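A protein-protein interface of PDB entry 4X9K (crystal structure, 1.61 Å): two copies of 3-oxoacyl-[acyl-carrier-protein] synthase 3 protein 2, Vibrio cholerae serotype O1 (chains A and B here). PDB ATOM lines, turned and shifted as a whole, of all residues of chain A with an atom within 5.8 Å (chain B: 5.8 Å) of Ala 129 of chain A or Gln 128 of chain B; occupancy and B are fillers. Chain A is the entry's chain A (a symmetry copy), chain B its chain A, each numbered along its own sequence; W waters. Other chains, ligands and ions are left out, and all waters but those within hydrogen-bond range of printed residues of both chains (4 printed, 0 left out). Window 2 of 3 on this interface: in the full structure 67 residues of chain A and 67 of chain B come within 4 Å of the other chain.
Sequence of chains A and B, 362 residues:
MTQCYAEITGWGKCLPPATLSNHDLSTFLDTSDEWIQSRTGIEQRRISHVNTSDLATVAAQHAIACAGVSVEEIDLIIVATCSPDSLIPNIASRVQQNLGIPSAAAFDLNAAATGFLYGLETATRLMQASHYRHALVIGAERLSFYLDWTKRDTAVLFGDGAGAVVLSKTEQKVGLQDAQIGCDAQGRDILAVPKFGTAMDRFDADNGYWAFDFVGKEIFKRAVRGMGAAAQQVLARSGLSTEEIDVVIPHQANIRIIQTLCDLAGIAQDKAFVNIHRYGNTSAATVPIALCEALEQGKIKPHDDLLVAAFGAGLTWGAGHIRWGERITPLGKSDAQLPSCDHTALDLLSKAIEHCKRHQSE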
ATOM      1  N   THR A 124       2.412   6.794  25.230  1.00  0.00           N
ATOM      2  CA  THR A 124       0.985   6.847  24.969  1.00  0.00           C
ATOM      3  C   THR A 124       0.393   5.454  25.184  1.00  0.00           C
ATOM      4  O   THR A 124      -0.614   5.318  25.857  1.00  0.00           O
ATOM      5  CB  THR A 124       0.679   7.356  23.555  1.00  0.00           C
ATOM      6  OG1 THR A 124       1.148   8.709  23.418  1.00  0.00           O
ATOM      7  CG2 THR A 124      -0.795   7.306  23.279  1.00  0.00           C
ATOM      8  N   ARG A 125       1.007   4.412  24.633  1.00  0.00           N
ATOM      9  CA  ARG A 125       0.435   3.085  24.797  1.00  0.00           C
ATOM     10  C   ARG A 125       0.551   2.554  26.232  1.00  0.00           C
ATOM     11  O   ARG A 125      -0.345   1.864  26.707  1.00  0.00           O
ATOM     12  CB  ARG A 125       1.052   2.085  23.823  1.00  0.00           C
ATOM     13  CG  ARG A 125       1.002   2.457  22.356  1.00  0.00           C
ATOM     14  CD  ARG A 125      -0.252   3.121  21.911  1.00  0.00           C
ATOM     15  NE  ARG A 125      -0.111   3.717  20.604  1.00  0.00           N
ATOM     16  CZ  ARG A 125      -1.059   4.368  19.973  1.00  0.00           C
ATOM     17  NH1 ARG A 125      -2.264   4.513  20.523  1.00  0.00           N
ATOM     18  NH2 ARG A 125      -0.768   4.927  18.793  1.00  0.00           N
ATOM     19  N   LEU A 126       1.655   2.847  26.919  1.00  0.00           N
ATOM     20  CA  LEU A 126       1.773   2.494  28.326  1.00  0.00           C
ATOM     21  C   LEU A 126       0.624   3.119  29.119  1.00  0.00           C
ATOM     22  O   LEU A 126       0.005   2.458  29.979  1.00  0.00           O
ATOM     23  CB  LEU A 126       3.115   2.956  28.889  1.00  0.00           C
ATOM     24  CG  LEU A 126       4.321   2.082  28.539  1.00  0.00           C
ATOM     25  CD1 LEU A 126       5.626   2.841  28.743  1.00  0.00           C
ATOM     26  CD2 LEU A 126       4.330   0.817  29.390  1.00  0.00           C
ATOM     27  N   MET A 127       0.327   4.388  28.835  1.00  0.00           N
ATOM     28  CA  MET A 127      -0.753   5.067  29.549  1.00  0.00           C
ATOM     29  C   MET A 127      -2.129   4.493  29.197  1.00  0.00           C
ATOM     30  O   MET A 127      -3.002   4.362  30.050  1.00  0.00           O
ATOM     31  CB  MET A 127      -0.707   6.568  29.252  1.00  0.00           C
ATOM     32  CG  MET A 127       0.484   7.255  29.887  1.00  0.00           C
ATOM     33  SD  MET A 127       0.811   8.939  29.328  1.00  0.00           S
ATOM     34  CE  MET A 127      -0.594   9.805  30.060  1.00  0.00           C
ATOM     35  N   GLN A 128      -2.323   4.125  27.941  1.00  0.00           N
ATOM     36  CA  GLN A 128      -3.596   3.573  27.511  1.00  0.00           C
ATOM     37  C   GLN A 128      -3.884   2.187  28.099  1.00  0.00           C
ATOM     38  O   GLN A 128      -5.036   1.862  28.413  1.00  0.00           O
ATOM     39  CB  GLN A 128      -3.646   3.523  25.995  1.00  0.00           C
ATOM     40  CG  GLN A 128      -3.799   4.915  25.408  1.00  0.00           C
ATOM     41  CD  GLN A 128      -3.812   4.953  23.896  1.00  0.00           C
ATOM     42  OE1 GLN A 128      -3.013   4.259  23.239  1.00  0.00           O
ATOM     43  NE2 GLN A 128      -4.685   5.778  23.328  1.00  0.00           N
ATOM     44  N   ALA A 129      -2.845   1.385  28.255  1.00  0.00           N
ATOM     45  CA  ALA A 129      -3.005   0.001  28.659  1.00  0.00           C
ATOM     46  C   ALA A 129      -2.755  -0.276  30.130  1.00  0.00           C
ATOM     47  O   ALA A 129      -3.060  -1.382  30.611  1.00  0.00           O
ATOM     48  CB  ALA A 129      -2.142  -0.901  27.789  1.00  0.00           C
ATOM     49  N   SER A 130      -2.213   0.684  30.861  1.00  0.00           N
ATOM     50  CA  SER A 130      -1.971   0.459  32.274  1.00  0.00           C
ATOM     51  C   SER A 130      -2.175   1.733  33.071  1.00  0.00           C
ATOM     52  O   SER A 130      -2.942   2.597  32.655  1.00  0.00           O
ATOM     53  CB  SER A 130      -0.602  -0.121  32.482  1.00  0.00           C
ATOM     54  OG  SER A 130      -0.512  -0.689  33.779  1.00  0.00           O
ATOM     55  N   HIS A 131      -1.532   1.829  34.230  1.00  0.00           N
ATOM     56  CA  HIS A 131      -1.971   2.789  35.254  1.00  0.00           C
ATOM     57  C   HIS A 131      -1.414   4.213  35.154  1.00  0.00           C
ATOM     58  O   HIS A 131      -1.947   5.108  35.816  1.00  0.00           O
ATOM     59  CB  HIS A 131      -1.646   2.230  36.646  1.00  0.00           C
ATOM     60  CG  HIS A 131      -0.186   2.019  36.857  1.00  0.00           C
ATOM     61  ND1 HIS A 131       0.687   3.059  37.122  1.00  0.00           N
ATOM     62  CD2 HIS A 131       0.573   0.901  36.781  1.00  0.00           C
ATOM     63  CE1 HIS A 131       1.916   2.580  37.222  1.00  0.00           C
ATOM     64  NE2 HIS A 131       1.875   1.280  36.992  1.00  0.00           N
ATOM     65  N   GLN B   3     -10.112  -6.797  24.880  1.00  0.00           N
ATOM     66  CA  GLN B   3      -8.887  -6.941  25.722  1.00  0.00           C
ATOM     67  C   GLN B   3      -7.993  -8.031  25.151  1.00  0.00           C
ATOM     68  O   GLN B   3      -8.428  -9.162  24.934  1.00  0.00           O
ATOM     69  CB  GLN B   3      -9.241  -7.266  27.178  1.00  0.00           C
ATOM     70  CG  GLN B   3      -8.045  -7.432  28.114  1.00  0.00           C
ATOM     71  CD  GLN B   3      -7.330  -6.126  28.406  1.00  0.00           C
ATOM     72  OE1 GLN B   3      -7.869  -5.255  29.094  1.00  0.00           O
ATOM     73  NE2 GLN B   3      -6.108  -5.984  27.897  1.00  0.00           N
ATOM     74  N   CYS B   4      -6.741  -7.649  24.896  1.00  0.00           N
ATOM     75  CA  CYS B   4      -5.722  -8.525  24.328  1.00  0.00           C
ATOM     76  C   CYS B   4      -4.603  -8.719  25.341  1.00  0.00           C
ATOM     77  O   CYS B   4      -4.509  -7.973  26.330  1.00  0.00           O
ATOM     78  CB  CYS B   4      -5.146  -7.911  23.057  1.00  0.00           C
ATOM     79  SG  CYS B   4      -6.281  -7.893  21.654  1.00  0.00           S
ATOM     80  N   TYR B   5      -3.761  -9.726  25.088  1.00  0.00           N
ATOM     81  CA  TYR B   5      -2.652 -10.077  25.962  1.00  0.00           C
ATOM     82  C   TYR B   5      -1.467 -10.455  25.089  1.00  0.00           C
ATOM     83  O   TYR B   5      -1.627 -10.719  23.889  1.00  0.00           O
ATOM     84  CB  TYR B   5      -3.062 -11.254  26.872  1.00  0.00           C
ATOM     85  CG  TYR B   5      -4.191 -10.899  27.815  1.00  0.00           C
ATOM     86  CD1 TYR B   5      -3.916 -10.294  29.025  1.00  0.00           C
ATOM     87  CD2 TYR B   5      -5.518 -11.126  27.468  1.00  0.00           C
ATOM     88  CE1 TYR B   5      -4.938  -9.933  29.893  1.00  0.00           C
ATOM     89  CE2 TYR B   5      -6.547 -10.775  28.325  1.00  0.00           C
ATOM     90  CZ  TYR B   5      -6.242 -10.180  29.534  1.00  0.00           C
ATOM     91  OH  TYR B   5      -7.255  -9.833  30.407  1.00  0.00           O
ATOM     92  N   ALA B   6      -0.292 -10.505  25.702  1.00  0.00           N
ATOM     93  CA  ALA B   6       0.952 -10.818  24.999  1.00  0.00           C
ATOM     94  C   ALA B   6       1.533 -12.103  25.597  1.00  0.00           C
ATOM     95  O   ALA B   6       2.233 -12.068  26.596  1.00  0.00           O
ATOM     96  CB  ALA B   6       1.934  -9.657  25.118  1.00  0.00           C
ATOM     97  N   ALA B 123       6.657  -3.802  25.771  1.00  0.00           N
ATOM     98  CA  ALA B 123       6.150  -4.555  24.630  1.00  0.00           C
ATOM     99  C   ALA B 123       4.711  -5.024  24.845  1.00  0.00           C
ATOM    100  O   ALA B 123       3.885  -4.993  23.928  1.00  0.00           O
ATOM    101  CB  ALA B 123       7.052  -5.739  24.338  1.00  0.00           C
ATOM    102  N   THR B 124       4.414  -5.479  26.060  1.00  0.00           N
ATOM    103  CA  THR B 124       3.084  -5.978  26.363  1.00  0.00           C
ATOM    104  C   THR B 124       2.077  -4.845  26.171  1.00  0.00           C
ATOM    105  O   THR B 124       1.059  -5.037  25.529  1.00  0.00           O
ATOM    106  CB  THR B 124       2.997  -6.551  27.782  1.00  0.00           C
ATOM    107  OG1 THR B 124       3.873  -7.687  27.900  1.00  0.00           O
ATOM    108  CG2 THR B 124       1.591  -6.968  28.102  1.00  0.00           C
ATOM    109  N   ARG B 125       2.347  -3.660  26.709  1.00  0.00           N
ATOM    110  CA  ARG B 125       1.380  -2.582  26.569  1.00  0.00           C
ATOM    111  C   ARG B 125       1.281  -2.048  25.133  1.00  0.00           C
ATOM    112  O   ARG B 125       0.199  -1.678  24.689  1.00  0.00           O
ATOM    113  CB  ARG B 125       1.678  -1.434  27.529  1.00  0.00           C
ATOM    114  CG  ARG B 125       1.791  -1.796  28.995  1.00  0.00           C
ATOM    115  CD  ARG B 125       0.825  -2.819  29.473  1.00  0.00           C
ATOM    116  NE  ARG B 125       1.185  -3.334  30.773  1.00  0.00           N
ATOM    117  CZ  ARG B 125       0.510  -4.248  31.429  1.00  0.00           C
ATOM    118  NH1 ARG B 125      -0.604  -4.769  30.913  1.00  0.00           N
ATOM    119  NH2 ARG B 125       0.997  -4.681  32.597  1.00  0.00           N
ATOM    120  N   LEU B 126       2.400  -1.981  24.413  1.00  0.00           N
ATOM    121  CA  LEU B 126       2.359  -1.615  23.005  1.00  0.00           C
ATOM    122  C   LEU B 126       1.443  -2.575  22.243  1.00  0.00           C
ATOM    123  O   LEU B 126       0.623  -2.148  21.405  1.00  0.00           O
ATOM    124  CB  LEU B 126       3.761  -1.633  22.400  1.00  0.00           C
ATOM    125  CG  LEU B 126       4.639  -0.421  22.719  1.00  0.00           C
ATOM    126  CD1 LEU B 126       6.110  -0.730  22.473  1.00  0.00           C
ATOM    127  CD2 LEU B 126       4.223   0.778  21.874  1.00  0.00           C
ATOM    128  N   MET B 127       1.570  -3.871  22.529  1.00  0.00           N
ATOM    129  CA  MET B 127       0.740  -4.861  21.844  1.00  0.00           C
ATOM    130  C   MET B 127      -0.737  -4.749  22.239  1.00  0.00           C
ATOM    131  O   MET B 127      -1.631  -4.904  21.413  1.00  0.00           O
ATOM    132  CB  MET B 127       1.266  -6.269  22.133  1.00  0.00           C
ATOM    133  CG  MET B 127       2.594  -6.547  21.460  1.00  0.00           C
ATOM    134  SD  MET B 127       3.452  -8.039  22.001  1.00  0.00           S
ATOM    135  CE  MET B 127       2.371  -9.309  21.306  1.00  0.00           C
ATOM    136  N   GLN B 128      -0.999  -4.455  23.502  1.00  0.00           N
ATOM    137  CA  GLN B 128      -2.369  -4.331  23.972  1.00  0.00           C
ATOM    138  C   GLN B 128      -3.096  -3.109  23.399  1.00  0.00           C
ATOM    139  O   GLN B 128      -4.301  -3.166  23.121  1.00  0.00           O
ATOM    140  CB  GLN B 128      -2.387  -4.291  25.489  1.00  0.00           C
ATOM    141  CG  GLN B 128      -2.075  -5.659  26.074  1.00  0.00           C
ATOM    142  CD  GLN B 128      -2.031  -5.691  27.586  1.00  0.00           C
ATOM    143  OE1 GLN B 128      -1.474  -4.777  28.221  1.00  0.00           O
ATOM    144  NE2 GLN B 128      -2.582  -6.747  28.175  1.00  0.00           N
ATOM    145  N   ALA B 129      -2.369  -2.021  23.217  1.00  0.00           N
ATOM    146  CA  ALA B 129      -2.970  -0.760  22.824  1.00  0.00           C
ATOM    147  C   ALA B 129      -2.863  -0.426  21.348  1.00  0.00           C
ATOM    148  O   ALA B 129      -3.516   0.525  20.881  1.00  0.00           O
ATOM    149  CB  ALA B 129      -2.410   0.372  23.673  1.00  0.00           C
ATOM    150  N   SER B 130      -2.068  -1.169  20.597  1.00  0.00           N
ATOM    151  CA  SER B 130      -1.951  -0.886  19.179  1.00  0.00           C
ATOM    152  C   SER B 130      -1.765  -2.163  18.382  1.00  0.00           C
ATOM    153  O   SER B 130      -2.208  -3.222  18.816  1.00  0.00           O
ATOM    154  CB  SER B 130      -0.841   0.096  18.933  1.00  0.00           C
ATOM    155  OG  SER B 130      -0.974   0.657  17.637  1.00  0.00           O
ATOM    156  N   LYS B 169       0.379 -11.906  20.356  1.00  0.00           N
ATOM    157  CA  LYS B 169      -0.929 -11.405  20.738  1.00  0.00           C
ATOM    158  C   LYS B 169      -1.981 -12.510  20.797  1.00  0.00           C
ATOM    159  O   LYS B 169      -2.061 -13.364  19.896  1.00  0.00           O
ATOM    160  CB  LYS B 169      -1.375 -10.334  19.750  1.00  0.00           C
ATOM    161  CG  LYS B 169      -2.697  -9.700  20.099  1.00  0.00           C
ATOM    162  CD  LYS B 169      -2.959  -8.502  19.209  1.00  0.00           C
ATOM    163  CE  LYS B 169      -2.160  -7.324  19.715  1.00  0.00           C
ATOM    164  NZ  LYS B 169      -2.429  -6.073  18.962  1.00  0.00           N
ATOM    165  N   LEU B 176       2.279 -11.379  30.645  1.00  0.00           N
ATOM    166  CA  LEU B 176       2.328 -10.363  31.707  1.00  0.00           C
ATOM    167  C   LEU B 176       0.944  -9.796  31.978  1.00  0.00           C
ATOM    168  O   LEU B 176       0.273  -9.284  31.087  1.00  0.00           O
ATOM    169  CB  LEU B 176       3.295  -9.236  31.318  1.00  0.00           C
ATOM    170  CG  LEU B 176       3.561  -8.183  32.425  1.00  0.00           C
ATOM    171  CD1 LEU B 176       4.361  -8.749  33.575  1.00  0.00           C
ATOM    172  CD2 LEU B 176       4.243  -6.971  31.822  1.00  0.00           C
HETATM  173  O   HOH W   1       0.774   2.455  17.018  1.00  0.00           O
HETATM  174  O   HOH W   2      -5.103   2.377  22.143  1.00  0.00           O
HETATM  175  O   HOH W   3      -4.017  -3.646  29.388  1.00  0.00           O
HETATM  176  O   HOH W   4       1.731  -1.840  34.337  1.00  0.00           O
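Of the 14 printed residues of chain B, 4 touch a printed residue of chain A.
Hydrophobic or aromatic side chains of chain B within 4 Å of the printed part of chain A: Leu 126 and Ala 129.
Printed residues of chain A that touch a printed residue of chain B: Arg 125, Leu 126, Gln 128 and Ala 129.
Hydrophobic or aromatic side chains of chain A that line the printed part of chain B: Leu 126 and Ala 129.
Among the printed residues, 7 pairs touch across the chains.
Of the printed residues of chain A, Gln 128 of chain B touches Ala 129 (3.96 Å).
Of the printed residues of chain B, Gln 128 of chain A touches Ala 129 (3.96 Å).
Of the printed residues of chain B, Arg 125 of chain A touches Arg 125 (3.95 Å), Leu 126 (3.7 Å) and Ala 129 (3.9 Å).
The nearest residue of chain B that does not touch Ala 129 of chain A is Ala 129 of chain B (4.3 Å).
The nearest printed residue of chain A that does not touch Arg 125 of chain B is Ser 130 of chain A (4.1 Å).
Water W1 lies within hydrogen-bond range of the side-chain hydroxyl of Ser 130 of chain B and the guanidinium group of Arg 125 of chain A.
Water W4 lies within hydrogen-bond range of OG of Ser 130 of chain A (2.6 Å) and NH2 of Arg 125 of chain B (3.4 Å).
Water W3 lies within hydrogen-bond range of O of Ala 129 of chain A (2.7 Å), OE1 of Gln 128 of chain B (3.0 Å) and NE2 of Gln 3 of chain B (3.5 Å).
Water W2 lies within hydrogen-bond range of O of Ala 129 of chain B (2.7 Å) and OE1 of Gln 128 of chain A (3.0 Å).
CB of Arg 125 of chain A touches O of Arg 125 of chain B (3.95 Å).
Arg 125 of chain A touches Leu 126 of chain B (CG to CD2, 3.7 Å).
Ala 129 of chain B touches Arg 125 of chain A.
CD2 of Leu 126 of chain A touches CG of Arg 125 of chain B (3.7 Å).
CB of Ala 129 of chain B touches OE1 of Gln 128 of chain A, 3.96 Å away.
Ala 129 of chain A touches Arg 125 of chain B.
Gln 128 of chain B touches Ala 129 of chain A (OE1 to CB, 3.96 Å).
The backbone carbonyl oxygen of Cys 4 of chain B lies within hydrogen-bond range of the side-chain amide nitrogen of Gln 128 of chain B (2.9 Å).
The side-chain amide oxygen (OE1) of Gln 128 of chain B sits at hydrogen-bond distance from the guanidinium group (NH1) of Arg 125 of chain B (2.8 Å).
The guanidinium group (NH1) of Arg 125 of chain A sits at hydrogen-bond distance from the side-chain amide oxygen (OE1) of Gln 128 of chain A (2.8 Å).
Arg 125 of chain B touches its own counterpart, Arg 125 of chain A.
Arg 125 of chain A touches Leu 126 of chain B, and with the chains exchanged Leu 126 of chain A touches Arg 125 of chain B.
Arg 125 of chain A touches Ala 129 of chain B, and with the chains exchanged Ala 129 of chain A touches Arg 125 of chain B.
Gln 128 of chain A touches Ala 129 of chain B, and with the chains exchanged Ala 129 of chain A touches Gln 128 of chain B.
Positions printed for both chains: 124, 125, 126, 127, 128, 129 and 130.
Of the 7 pairs that touch across the chains among the printed residues, 7 have their exchanged pair printed and touching as well.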
